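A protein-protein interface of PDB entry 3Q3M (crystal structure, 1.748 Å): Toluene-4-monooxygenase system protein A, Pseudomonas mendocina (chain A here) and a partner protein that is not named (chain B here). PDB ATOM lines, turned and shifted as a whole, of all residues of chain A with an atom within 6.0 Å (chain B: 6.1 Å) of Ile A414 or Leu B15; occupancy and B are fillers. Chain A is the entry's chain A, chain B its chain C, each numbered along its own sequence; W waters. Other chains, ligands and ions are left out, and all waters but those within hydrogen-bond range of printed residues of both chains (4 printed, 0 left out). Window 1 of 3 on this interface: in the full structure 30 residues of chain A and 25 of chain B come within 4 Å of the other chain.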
ATOM      1  N   GLY A 334     -22.025  -0.691  -7.787  1.00  0.00           N
ATOM      2  CA  GLY A 334     -21.476  -0.598  -6.429  1.00  0.00           C
ATOM      3  C   GLY A 334     -20.597   0.617  -6.179  1.00  0.00           C
ATOM      4  O   GLY A 334     -20.740   1.331  -5.170  1.00  0.00           O
ATOM      5  N   TRP A 338     -21.905   3.563  -3.659  1.00  0.00           N
ATOM      6  CA  TRP A 338     -20.987   3.860  -2.559  1.00  0.00           C
ATOM      7  C   TRP A 338     -19.909   4.888  -2.968  1.00  0.00           C
ATOM      8  O   TRP A 338     -18.797   4.887  -2.454  1.00  0.00           O
ATOM      9  CB  TRP A 338     -20.358   2.552  -2.004  1.00  0.00           C
ATOM     10  CG  TRP A 338     -21.282   1.834  -1.031  1.00  0.00           C
ATOM     11  CD1 TRP A 338     -21.256   1.906   0.330  1.00  0.00           C
ATOM     12  CD2 TRP A 338     -22.363   0.949  -1.366  1.00  0.00           C
ATOM     13  NE1 TRP A 338     -22.268   1.131   0.869  1.00  0.00           N
ATOM     14  CE2 TRP A 338     -22.950   0.524  -0.150  1.00  0.00           C
ATOM     15  CE3 TRP A 338     -22.885   0.465  -2.581  1.00  0.00           C
ATOM     16  CZ2 TRP A 338     -24.044  -0.340  -0.105  1.00  0.00           C
ATOM     17  CZ3 TRP A 338     -23.973  -0.388  -2.538  1.00  0.00           C
ATOM     18  CH2 TRP A 338     -24.540  -0.793  -1.301  1.00  0.00           C
ATOM     19  N   PRO A 394     -21.420  -2.765   1.856  1.00  0.00           N
ATOM     20  CA  PRO A 394     -21.592  -3.943   0.998  1.00  0.00           C
ATOM     21  C   PRO A 394     -20.810  -5.098   1.611  1.00  0.00           C
ATOM     22  O   PRO A 394     -19.798  -4.820   2.287  1.00  0.00           O
ATOM     23  CB  PRO A 394     -20.924  -3.513  -0.314  1.00  0.00           C
ATOM     24  CG  PRO A 394     -19.911  -2.500   0.084  1.00  0.00           C
ATOM     25  CD  PRO A 394     -20.423  -1.814   1.322  1.00  0.00           C
ATOM     26  N   SER A 395     -21.263  -6.345   1.406  1.00  0.00           N
ATOM     27  CA  SER A 395     -20.470  -7.526   1.748  1.00  0.00           C
ATOM     28  C   SER A 395     -19.303  -7.625   0.758  1.00  0.00           C
ATOM     29  O   SER A 395     -19.485  -7.326  -0.423  1.00  0.00           O
ATOM     30  CB  SER A 395     -21.341  -8.788   1.652  1.00  0.00           C
ATOM     31  OG  SER A 395     -22.543  -8.619   2.388  1.00  0.00           O
ATOM     32  N   PRO A 403     -16.860  -5.730  -3.518  1.00  0.00           N
ATOM     33  CA  PRO A 403     -18.195  -6.200  -3.110  1.00  0.00           C
ATOM     34  C   PRO A 403     -18.710  -7.445  -3.819  1.00  0.00           C
ATOM     35  O   PRO A 403     -18.452  -7.665  -5.026  1.00  0.00           O
ATOM     36  CB  PRO A 403     -19.099  -4.990  -3.431  1.00  0.00           C
ATOM     37  CG  PRO A 403     -18.215  -3.818  -3.164  1.00  0.00           C
ATOM     38  CD  PRO A 403     -16.813  -4.260  -3.641  1.00  0.00           C
ATOM     39  N   LEU A 404     -19.469  -8.248  -3.070  1.00  0.00           N
ATOM     40  CA  LEU A 404     -20.073  -9.459  -3.616  1.00  0.00           C
ATOM     41  C   LEU A 404     -21.311  -9.078  -4.448  1.00  0.00           C
ATOM     42  O   LEU A 404     -22.262  -8.512  -3.922  1.00  0.00           O
ATOM     43  CB  LEU A 404     -20.456 -10.384  -2.469  1.00  0.00           C
ATOM     44  CG  LEU A 404     -19.265 -10.798  -1.609  1.00  0.00           C
ATOM     45  CD1 LEU A 404     -19.750 -11.572  -0.361  1.00  0.00           C
ATOM     46  CD2 LEU A 404     -18.365 -11.664  -2.474  1.00  0.00           C
ATOM     47  N   VAL A 405     -21.290  -9.374  -5.748  1.00  0.00           N
ATOM     48  CA  VAL A 405     -22.365  -8.915  -6.628  1.00  0.00           C
ATOM     49  C   VAL A 405     -22.953 -10.060  -7.448  1.00  0.00           C
ATOM     50  O   VAL A 405     -22.439 -11.181  -7.432  1.00  0.00           O
ATOM     51  CB  VAL A 405     -21.873  -7.775  -7.588  1.00  0.00           C
ATOM     52  CG1 VAL A 405     -21.270  -6.610  -6.792  1.00  0.00           C
ATOM     53  CG2 VAL A 405     -20.822  -8.305  -8.605  1.00  0.00           C
ATOM     54  N   GLY A 406     -24.018  -9.760  -8.192  1.00  0.00           N
ATOM     55  CA  GLY A 406     -24.600 -10.727  -9.102  1.00  0.00           C
ATOM     56  C   GLY A 406     -25.382  -9.963 -10.145  1.00  0.00           C
ATOM     57  O   GLY A 406     -25.174  -8.754 -10.332  1.00  0.00           O
ATOM     58  N   VAL A 407     -26.303 -10.647 -10.799  1.00  0.00           N
ATOM     59  CA  VAL A 407     -27.118 -10.031 -11.837  1.00  0.00           C
ATOM     60  C   VAL A 407     -28.448  -9.645 -11.211  1.00  0.00           C
ATOM     61  O   VAL A 407     -29.135 -10.504 -10.671  1.00  0.00           O
ATOM     62  CB  VAL A 407     -27.374 -11.036 -12.979  1.00  0.00           C
ATOM     63  CG1 VAL A 407     -28.324 -10.424 -14.034  1.00  0.00           C
ATOM     64  CG2 VAL A 407     -26.054 -11.453 -13.627  1.00  0.00           C
ATOM     65  N   TRP A 412     -32.797 -12.220 -11.729  1.00  0.00           N
ATOM     66  CA  TRP A 412     -31.908 -12.109 -10.581  1.00  0.00           C
ATOM     67  C   TRP A 412     -31.160 -13.399 -10.290  1.00  0.00           C
ATOM     68  O   TRP A 412     -31.765 -14.462 -10.136  1.00  0.00           O
ATOM     69  CB  TRP A 412     -32.755 -11.762  -9.361  1.00  0.00           C
ATOM     70  CG  TRP A 412     -32.009 -11.650  -8.088  1.00  0.00           C
ATOM     71  CD1 TRP A 412     -31.023 -10.751  -7.787  1.00  0.00           C
ATOM     72  CD2 TRP A 412     -32.239 -12.410  -6.895  1.00  0.00           C
ATOM     73  NE1 TRP A 412     -30.605 -10.927  -6.476  1.00  0.00           N
ATOM     74  CE2 TRP A 412     -31.335 -11.939  -5.910  1.00  0.00           C
ATOM     75  CE3 TRP A 412     -33.107 -13.458  -6.568  1.00  0.00           C
ATOM     76  CZ2 TRP A 412     -31.283 -12.479  -4.612  1.00  0.00           C
ATOM     77  CZ3 TRP A 412     -33.057 -13.990  -5.289  1.00  0.00           C
ATOM     78  CH2 TRP A 412     -32.148 -13.503  -4.324  1.00  0.00           C
ATOM     79  N   ASN A 413     -29.842 -13.306 -10.234  1.00  0.00           N
ATOM     80  CA  ASN A 413     -29.041 -14.417  -9.771  1.00  0.00           C
ATOM     81  C   ASN A 413     -27.814 -13.893  -9.092  1.00  0.00           C
ATOM     82  O   ASN A 413     -27.076 -13.094  -9.661  1.00  0.00           O
ATOM     83  CB  ASN A 413     -28.628 -15.353 -10.901  1.00  0.00           C
ATOM     84  CG  ASN A 413     -27.896 -16.589 -10.370  1.00  0.00           C
ATOM     85  OD1 ASN A 413     -28.486 -17.425  -9.686  1.00  0.00           O
ATOM     86  ND2 ASN A 413     -26.607 -16.671 -10.634  1.00  0.00           N
ATOM     87  N   ILE A 414     -27.611 -14.313  -7.855  1.00  0.00           N
ATOM     88  CA  ILE A 414     -26.416 -13.903  -7.127  1.00  0.00           C
ATOM     89  C   ILE A 414     -25.903 -15.085  -6.319  1.00  0.00           C
ATOM     90  O   ILE A 414     -26.699 -15.824  -5.737  1.00  0.00           O
ATOM     91  CB  ILE A 414     -26.679 -12.676  -6.240  1.00  0.00           C
ATOM     92  CG1 ILE A 414     -25.376 -12.203  -5.574  1.00  0.00           C
ATOM     93  CG2 ILE A 414     -27.778 -12.947  -5.200  1.00  0.00           C
ATOM     94  CD1 ILE A 414     -25.429 -10.720  -5.196  1.00  0.00           C
ATOM     95  N   GLU A 415     -24.588 -15.294  -6.322  1.00  0.00           N
ATOM     96  CA  GLU A 415     -24.017 -16.414  -5.570  1.00  0.00           C
ATOM     97  C   GLU A 415     -22.733 -16.038  -4.848  1.00  0.00           C
ATOM     98  O   GLU A 415     -21.806 -15.479  -5.447  1.00  0.00           O
ATOM     99  CB  GLU A 415     -23.747 -17.649  -6.446  1.00  0.00           C
ATOM    100  CG  GLU A 415     -23.313 -18.871  -5.577  1.00  0.00           C
ATOM    101  CD  GLU A 415     -23.506 -20.223  -6.264  1.00  0.00           C
ATOM    102  OE1 GLU A 415     -23.869 -20.253  -7.464  1.00  0.00           O
ATOM    103  OE2 GLU A 415     -23.311 -21.251  -5.579  1.00  0.00           O
ATOM    104  N   VAL A 416     -22.694 -16.367  -3.563  1.00  0.00           N
ATOM    105  CA  VAL A 416     -21.492 -16.229  -2.742  1.00  0.00           C
ATOM    106  C   VAL A 416     -20.946 -17.635  -2.497  1.00  0.00           C
ATOM    107  O   VAL A 416     -21.699 -18.575  -2.211  1.00  0.00           O
ATOM    108  CB  VAL A 416     -21.845 -15.568  -1.388  1.00  0.00           C
ATOM    109  CG1 VAL A 416     -20.626 -15.432  -0.487  1.00  0.00           C
ATOM    110  CG2 VAL A 416     -22.504 -14.222  -1.629  1.00  0.00           C
ATOM    111  N   ALA B   8     -26.741 -10.250   3.591  1.00  0.00           N
ATOM    112  CA  ALA B   8     -28.060 -10.522   3.023  1.00  0.00           C
ATOM    113  C   ALA B   8     -28.146 -10.151   1.539  1.00  0.00           C
ATOM    114  O   ALA B   8     -27.650  -9.112   1.101  1.00  0.00           O
ATOM    115  CB  ALA B   8     -29.193  -9.802   3.857  1.00  0.00           C
ATOM    116  N   ALA B   9     -28.759 -11.033   0.763  1.00  0.00           N
ATOM    117  CA  ALA B   9     -28.989 -10.785  -0.656  1.00  0.00           C
ATOM    118  C   ALA B   9     -30.494 -10.635  -0.864  1.00  0.00           C
ATOM    119  O   ALA B   9     -31.248 -11.599  -0.678  1.00  0.00           O
ATOM    120  CB  ALA B   9     -28.436 -11.946  -1.491  1.00  0.00           C
ATOM    121  N   PHE B  10     -30.933  -9.432  -1.241  1.00  0.00           N
ATOM    122  CA  PHE B  10     -32.360  -9.186  -1.457  1.00  0.00           C
ATOM    123  C   PHE B  10     -32.768  -9.450  -2.915  1.00  0.00           C
ATOM    124  O   PHE B  10     -32.064  -9.072  -3.840  1.00  0.00           O
ATOM    125  CB  PHE B  10     -32.706  -7.750  -1.094  1.00  0.00           C
ATOM    126  CG  PHE B  10     -34.183  -7.519  -0.892  1.00  0.00           C
ATOM    127  CD1 PHE B  10     -35.000  -7.204  -1.963  1.00  0.00           C
ATOM    128  CD2 PHE B  10     -34.741  -7.600   0.371  1.00  0.00           C
ATOM    129  CE1 PHE B  10     -36.378  -6.991  -1.769  1.00  0.00           C
ATOM    130  CE2 PHE B  10     -36.102  -7.369   0.576  1.00  0.00           C
ATOM    131  CZ  PHE B  10     -36.922  -7.081  -0.494  1.00  0.00           C
ATOM    132  N   ASP B  13     -31.953  -7.352  -6.313  1.00  0.00           N
ATOM    133  CA  ASP B  13     -30.836  -6.417  -6.050  1.00  0.00           C
ATOM    134  C   ASP B  13     -29.590  -6.921  -6.775  1.00  0.00           C
ATOM    135  O   ASP B  13     -29.579  -8.033  -7.323  1.00  0.00           O
ATOM    136  CB  ASP B  13     -30.568  -6.293  -4.541  1.00  0.00           C
ATOM    137  CG  ASP B  13     -29.967  -4.937  -4.140  1.00  0.00           C
ATOM    138  OD1 ASP B  13     -29.633  -4.103  -5.014  1.00  0.00           O
ATOM    139  OD2 ASP B  13     -29.828  -4.706  -2.926  1.00  0.00           O
ATOM    140  N   PHE B  14     -28.529  -6.122  -6.767  1.00  0.00           N
ATOM    141  CA  PHE B  14     -27.310  -6.486  -7.483  1.00  0.00           C
ATOM    142  C   PHE B  14     -26.175  -6.970  -6.571  1.00  0.00           C
ATOM    143  O   PHE B  14     -25.101  -7.344  -7.069  1.00  0.00           O
ATOM    144  CB  PHE B  14     -26.802  -5.301  -8.310  1.00  0.00           C
ATOM    145  CG  PHE B  14     -25.953  -4.316  -7.513  1.00  0.00           C
ATOM    146  CD1 PHE B  14     -24.578  -4.376  -7.575  1.00  0.00           C
ATOM    147  CD2 PHE B  14     -26.548  -3.352  -6.689  1.00  0.00           C
ATOM    148  CE1 PHE B  14     -23.781  -3.473  -6.853  1.00  0.00           C
ATOM    149  CE2 PHE B  14     -25.772  -2.448  -5.954  1.00  0.00           C
ATOM    150  CZ  PHE B  14     -24.384  -2.508  -6.033  1.00  0.00           C
ATOM    151  N   LEU B  15     -26.375  -6.917  -5.250  1.00  0.00           N
ATOM    152  CA  LEU B  15     -25.287  -7.253  -4.328  1.00  0.00           C
ATOM    153  C   LEU B  15     -25.771  -7.910  -3.038  1.00  0.00           C
ATOM    154  O   LEU B  15     -26.979  -8.023  -2.794  1.00  0.00           O
ATOM    155  CB  LEU B  15     -24.453  -6.025  -3.977  1.00  0.00           C
ATOM    156  CG  LEU B  15     -24.887  -5.136  -2.802  1.00  0.00           C
ATOM    157  CD1 LEU B  15     -23.852  -4.014  -2.586  1.00  0.00           C
ATOM    158  CD2 LEU B  15     -26.302  -4.532  -2.938  1.00  0.00           C
ATOM    159  N   VAL B  16     -24.801  -8.343  -2.245  1.00  0.00           N
ATOM    160  CA  VAL B  16     -25.011  -8.809  -0.885  1.00  0.00           C
ATOM    161  C   VAL B  16     -24.525  -7.685   0.038  1.00  0.00           C
ATOM    162  O   VAL B  16     -23.496  -7.079  -0.237  1.00  0.00           O
ATOM    163  CB  VAL B  16     -24.193 -10.081  -0.634  1.00  0.00           C
ATOM    164  CG1 VAL B  16     -24.520 -10.689   0.738  1.00  0.00           C
ATOM    165  CG2 VAL B  16     -24.423 -11.108  -1.783  1.00  0.00           C
ATOM    166  N   GLN B  17     -25.292  -7.376   1.089  1.00  0.00           N
ATOM    167  CA  GLN B  17     -24.900  -6.335   2.057  1.00  0.00           C
ATOM    168  C   GLN B  17     -24.797  -6.854   3.481  1.00  0.00           C
ATOM    169  O   GLN B  17     -25.497  -7.794   3.862  1.00  0.00           O
ATOM    170  CB  GLN B  17     -25.923  -5.208   2.066  1.00  0.00           C
ATOM    171  CG  GLN B  17     -25.991  -4.406   0.773  1.00  0.00           C
ATOM    172  CD  GLN B  17     -27.129  -3.409   0.780  1.00  0.00           C
ATOM    173  OE1 GLN B  17     -28.306  -3.776   0.924  1.00  0.00           O
ATOM    174  NE2 GLN B  17     -26.793  -2.147   0.615  1.00  0.00           N
ATOM    175  N   CYS B  38     -32.654  -1.775   0.537  1.00  0.00           N
ATOM    176  CA  CYS B  38     -32.817  -2.315  -0.822  1.00  0.00           C
ATOM    177  C   CYS B  38     -34.040  -1.775  -1.554  1.00  0.00           C
ATOM    178  O   CYS B  38     -33.923  -1.214  -2.643  1.00  0.00           O
ATOM    179  CB  CYS B  38     -32.917  -3.845  -0.786  1.00  0.00           C
ATOM    180  SG  CYS B  38     -31.505  -4.659  -0.042  1.00  0.00           S
ATOM    181  N   ARG B  42     -32.705   0.376  -4.866  1.00  0.00           N
ATOM    182  CA  ARG B  42     -32.328  -0.242  -6.136  1.00  0.00           C
ATOM    183  C   ARG B  42     -33.367  -1.297  -6.560  1.00  0.00           C
ATOM    184  O   ARG B  42     -33.246  -1.894  -7.629  1.00  0.00           O
ATOM    185  CB  ARG B  42     -30.930  -0.872  -6.040  1.00  0.00           C
ATOM    186  CG  ARG B  42     -29.781   0.132  -5.691  1.00  0.00           C
ATOM    187  CD  ARG B  42     -28.460  -0.609  -5.388  1.00  0.00           C
ATOM    188  NE  ARG B  42     -28.708  -1.561  -4.310  1.00  0.00           N
ATOM    189  CZ  ARG B  42     -28.653  -1.261  -3.019  1.00  0.00           C
ATOM    190  NH1 ARG B  42     -28.967  -2.187  -2.118  1.00  0.00           N
ATOM    191  NH2 ARG B  42     -28.273  -0.050  -2.623  1.00  0.00           N
ATOM    192  N   HIS B  55     -28.624 -18.751   2.232  1.00  0.00           N
ATOM    193  CA  HIS B  55     -28.224 -18.441   0.867  1.00  0.00           C
ATOM    194  C   HIS B  55     -28.323 -19.650  -0.072  1.00  0.00           C
ATOM    195  O   HIS B  55     -27.788 -20.712   0.224  1.00  0.00           O
ATOM    196  CB  HIS B  55     -26.794 -17.888   0.869  1.00  0.00           C
ATOM    197  CG  HIS B  55     -26.333 -17.388  -0.465  1.00  0.00           C
ATOM    198  ND1 HIS B  55     -27.084 -16.529  -1.241  1.00  0.00           N
ATOM    199  CD2 HIS B  55     -25.186 -17.608  -1.148  1.00  0.00           C
ATOM    200  CE1 HIS B  55     -26.421 -16.253  -2.350  1.00  0.00           C
ATOM    201  NE2 HIS B  55     -25.267 -16.896  -2.320  1.00  0.00           N
ATOM    202  N   ARG B  56     -29.015 -19.457  -1.194  1.00  0.00           N
ATOM    203  CA  ARG B  56     -29.230 -20.472  -2.234  1.00  0.00           C
ATOM    204  C   ARG B  56     -29.946 -21.724  -1.753  1.00  0.00           C
ATOM    205  O   ARG B  56     -29.945 -22.728  -2.464  1.00  0.00           O
ATOM    206  CB  ARG B  56     -27.911 -20.903  -2.892  1.00  0.00           C
ATOM    207  CG  ARG B  56     -26.911 -19.795  -3.201  1.00  0.00           C
ATOM    208  CD  ARG B  56     -27.121 -19.106  -4.557  1.00  0.00           C
ATOM    209  NE  ARG B  56     -27.172 -20.006  -5.714  1.00  0.00           N
ATOM    210  CZ  ARG B  56     -27.453 -19.585  -6.943  1.00  0.00           C
ATOM    211  NH1 ARG B  56     -27.700 -18.291  -7.152  1.00  0.00           N
ATOM    212  NH2 ARG B  56     -27.492 -20.441  -7.961  1.00  0.00           N
ATOM    213  N   ASP B  79     -30.723 -15.098   1.968  1.00  0.00           N
ATOM    214  CA  ASP B  79     -31.493 -14.390   0.946  1.00  0.00           C
ATOM    215  C   ASP B  79     -32.815 -13.933   1.519  1.00  0.00           C
ATOM    216  O   ASP B  79     -33.399 -14.615   2.361  1.00  0.00           O
ATOM    217  CB  ASP B  79     -31.834 -15.293  -0.244  1.00  0.00           C
ATOM    218  CG  ASP B  79     -30.604 -15.933  -0.894  1.00  0.00           C
ATOM    219  OD1 ASP B  79     -29.501 -15.359  -0.840  1.00  0.00           O
ATOM    220  OD2 ASP B  79     -30.751 -17.028  -1.468  1.00  0.00           O
HETATM  221  O   HOH W   1     -27.562  -9.802  -7.953  1.00  0.00           O
HETATM  222  O   HOH W   2     -27.937 -20.475 -10.767  1.00  0.00           O
HETATM  223  O   HOH W   3     -29.734 -16.431  -4.142  1.00  0.00           O
HETATM  224  O   HOH W   4     -29.278  -9.584  -4.191  1.00  0.00           O
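Water W1 lies within hydrogen-bond range of the backbone carbonyl oxygen of Asp B13 (2.8 Å) and the backbone carbonyl oxygen of Val A407 (3.2 Å).
Water W2 lies within hydrogen-bond range of the guanidinium group (NH2) of Arg B56 (2.8 Å) and the side-chain amide oxygen (OD1) of Asn A413 (3.3 Å).
Water W4 lies within hydrogen-bond range of O of Phe B10 (2.9 Å), NE1 of Trp A412 (3.0 Å) and O of Leu B15 (3.1 Å).
Water W3 lies within hydrogen-bond range of the side-chain carboxylate (OD2) of Asp B79 (2.9 Å) and the backbone carbonyl oxygen (O) of Ile A414 (3.5 Å).
N of Val A407 is in hydrogen-bond range of O of Asn A413 (2.8 Å).
The side-chain sulfur (SG) of Cys B38 is in hydrogen-bond range of the side-chain carboxylate (OD2) of Asp B13 (3.3 Å).
The guanidinium group (NH1) of Arg B42 lies within salt-bridge range of the side-chain carboxylate (OD2) of Asp B13 (2.8 Å).
The side-chain amide oxygen (OE1) of Gln B17 sits at hydrogen-bond distance from the side-chain sulfur (SG) of Cys B38.
The side-chain amide nitrogen of Gln B17 lies close to the guanidinium group of Arg B42, at 3.5 Å.
OD1 of Asp B79 sits at hydrogen-bond distance from ND1 of His B55 (2.7 Å).
Of the 13 printed residues of chain B, 9 touch a printed residue of chain A.
Printed residues of chain B that touch a printed residue of chain A: Ala B9, Phe B10, Asp B13, Phe B14, Leu B15, Val B16, Gln B17, His B55 and Arg B56.
Printed residues of chain A that touch a printed residue of chain B: Gly A334, Trp A338, Pro A394, Ser A395, Leu A404, Val A405, Gly A406, Trp A412, Asn A413, Ile A414, Glu A415 and Val A416.
Among the printed residues, 24 pairs touch across the chains.
Among the printed residues, Asp or Glu carboxylates within 4 Å of a Lys or Arg side-chain nitrogen of the other chain: Glu A415 with Arg B56 (3.7 Å).
The backbone carbonyl oxygen of Val B16 is in hydrogen-bond range of the backbone NH of Ser A395, at 2.9 Å.
The backbone NH of Gln B17 lies close to the side-chain hydroxyl of Ser A395, at 3.3 Å.
O of Leu A404 is in hydrogen-bond range of N of Val B16 (3.0 Å).
O of Phe B14 lies within hydrogen-bond range of N of Gly A406.
The indole nitrogen of Trp A412 lies close to the backbone carbonyl oxygen of Asp B13 (3.2 Å).
The guanidinium group (NH1) of Arg B56 lies within hydrogen-bond range of the side-chain amide oxygen (OD1) of Asn A413, 2.8 Å away.
The backbone carbonyl oxygen (O) of Ile A414 sits at hydrogen-bond distance from the guanidinium group (NH1) of Arg B56.
OE1 of Glu A415 lies within salt-bridge range of NH2 of Arg B56, at 3.7 Å.
The backbone NH (N) of Val A416 lies within hydrogen-bond range of a ring nitrogen (NE2) of His B55, at 2.9 Å.
Of the printed residues of chain A, Leu B15 touches Trp A338 (3.5 Å), Pro A394 (3.7 Å), Leu A404 (3.3 Å) and Ile A414 (3.6 Å).
Printed residues of chain B within 4 Å of Gly A406: Phe B14.
Printed residues of chain B within 4 Å of Val A405: Phe B14.
The nearest residue of chain A that does not touch Leu B15 is Val A405 (4.1 Å).
The nearest printed residue of chain A that does not touch Phe B10 is Ile A414 (5.9 Å).
Among the printed residues, pairs that only touch across the chains: Gly A334 with Phe B14 (3.4 Å), Trp A338 with Leu B15 (3.5 Å), Trp A338 with Gln B17 (3.3 Å), Pro A394 with Leu B15 (3.7 Å), Pro A394 with Val B16 (3.8 Å), Leu A404 with Leu B15 (3.3 Å), Val A405 with Phe B14 (3.2 Å), Trp A412 with Phe B10 (3.5 Å), Ile A414 with Ala B9 (3.9 Å), Ile A414 with Phe B14 (3.9 Å), Ile A414 with Leu B15 (3.6 Å), Ile A414 with Val B16 (3.6 Å), Ile A414 with His B55 (3.4 Å), Glu A415 with His B55 (3.5 Å) and Val A416 with Val B16 (3.7 Å).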
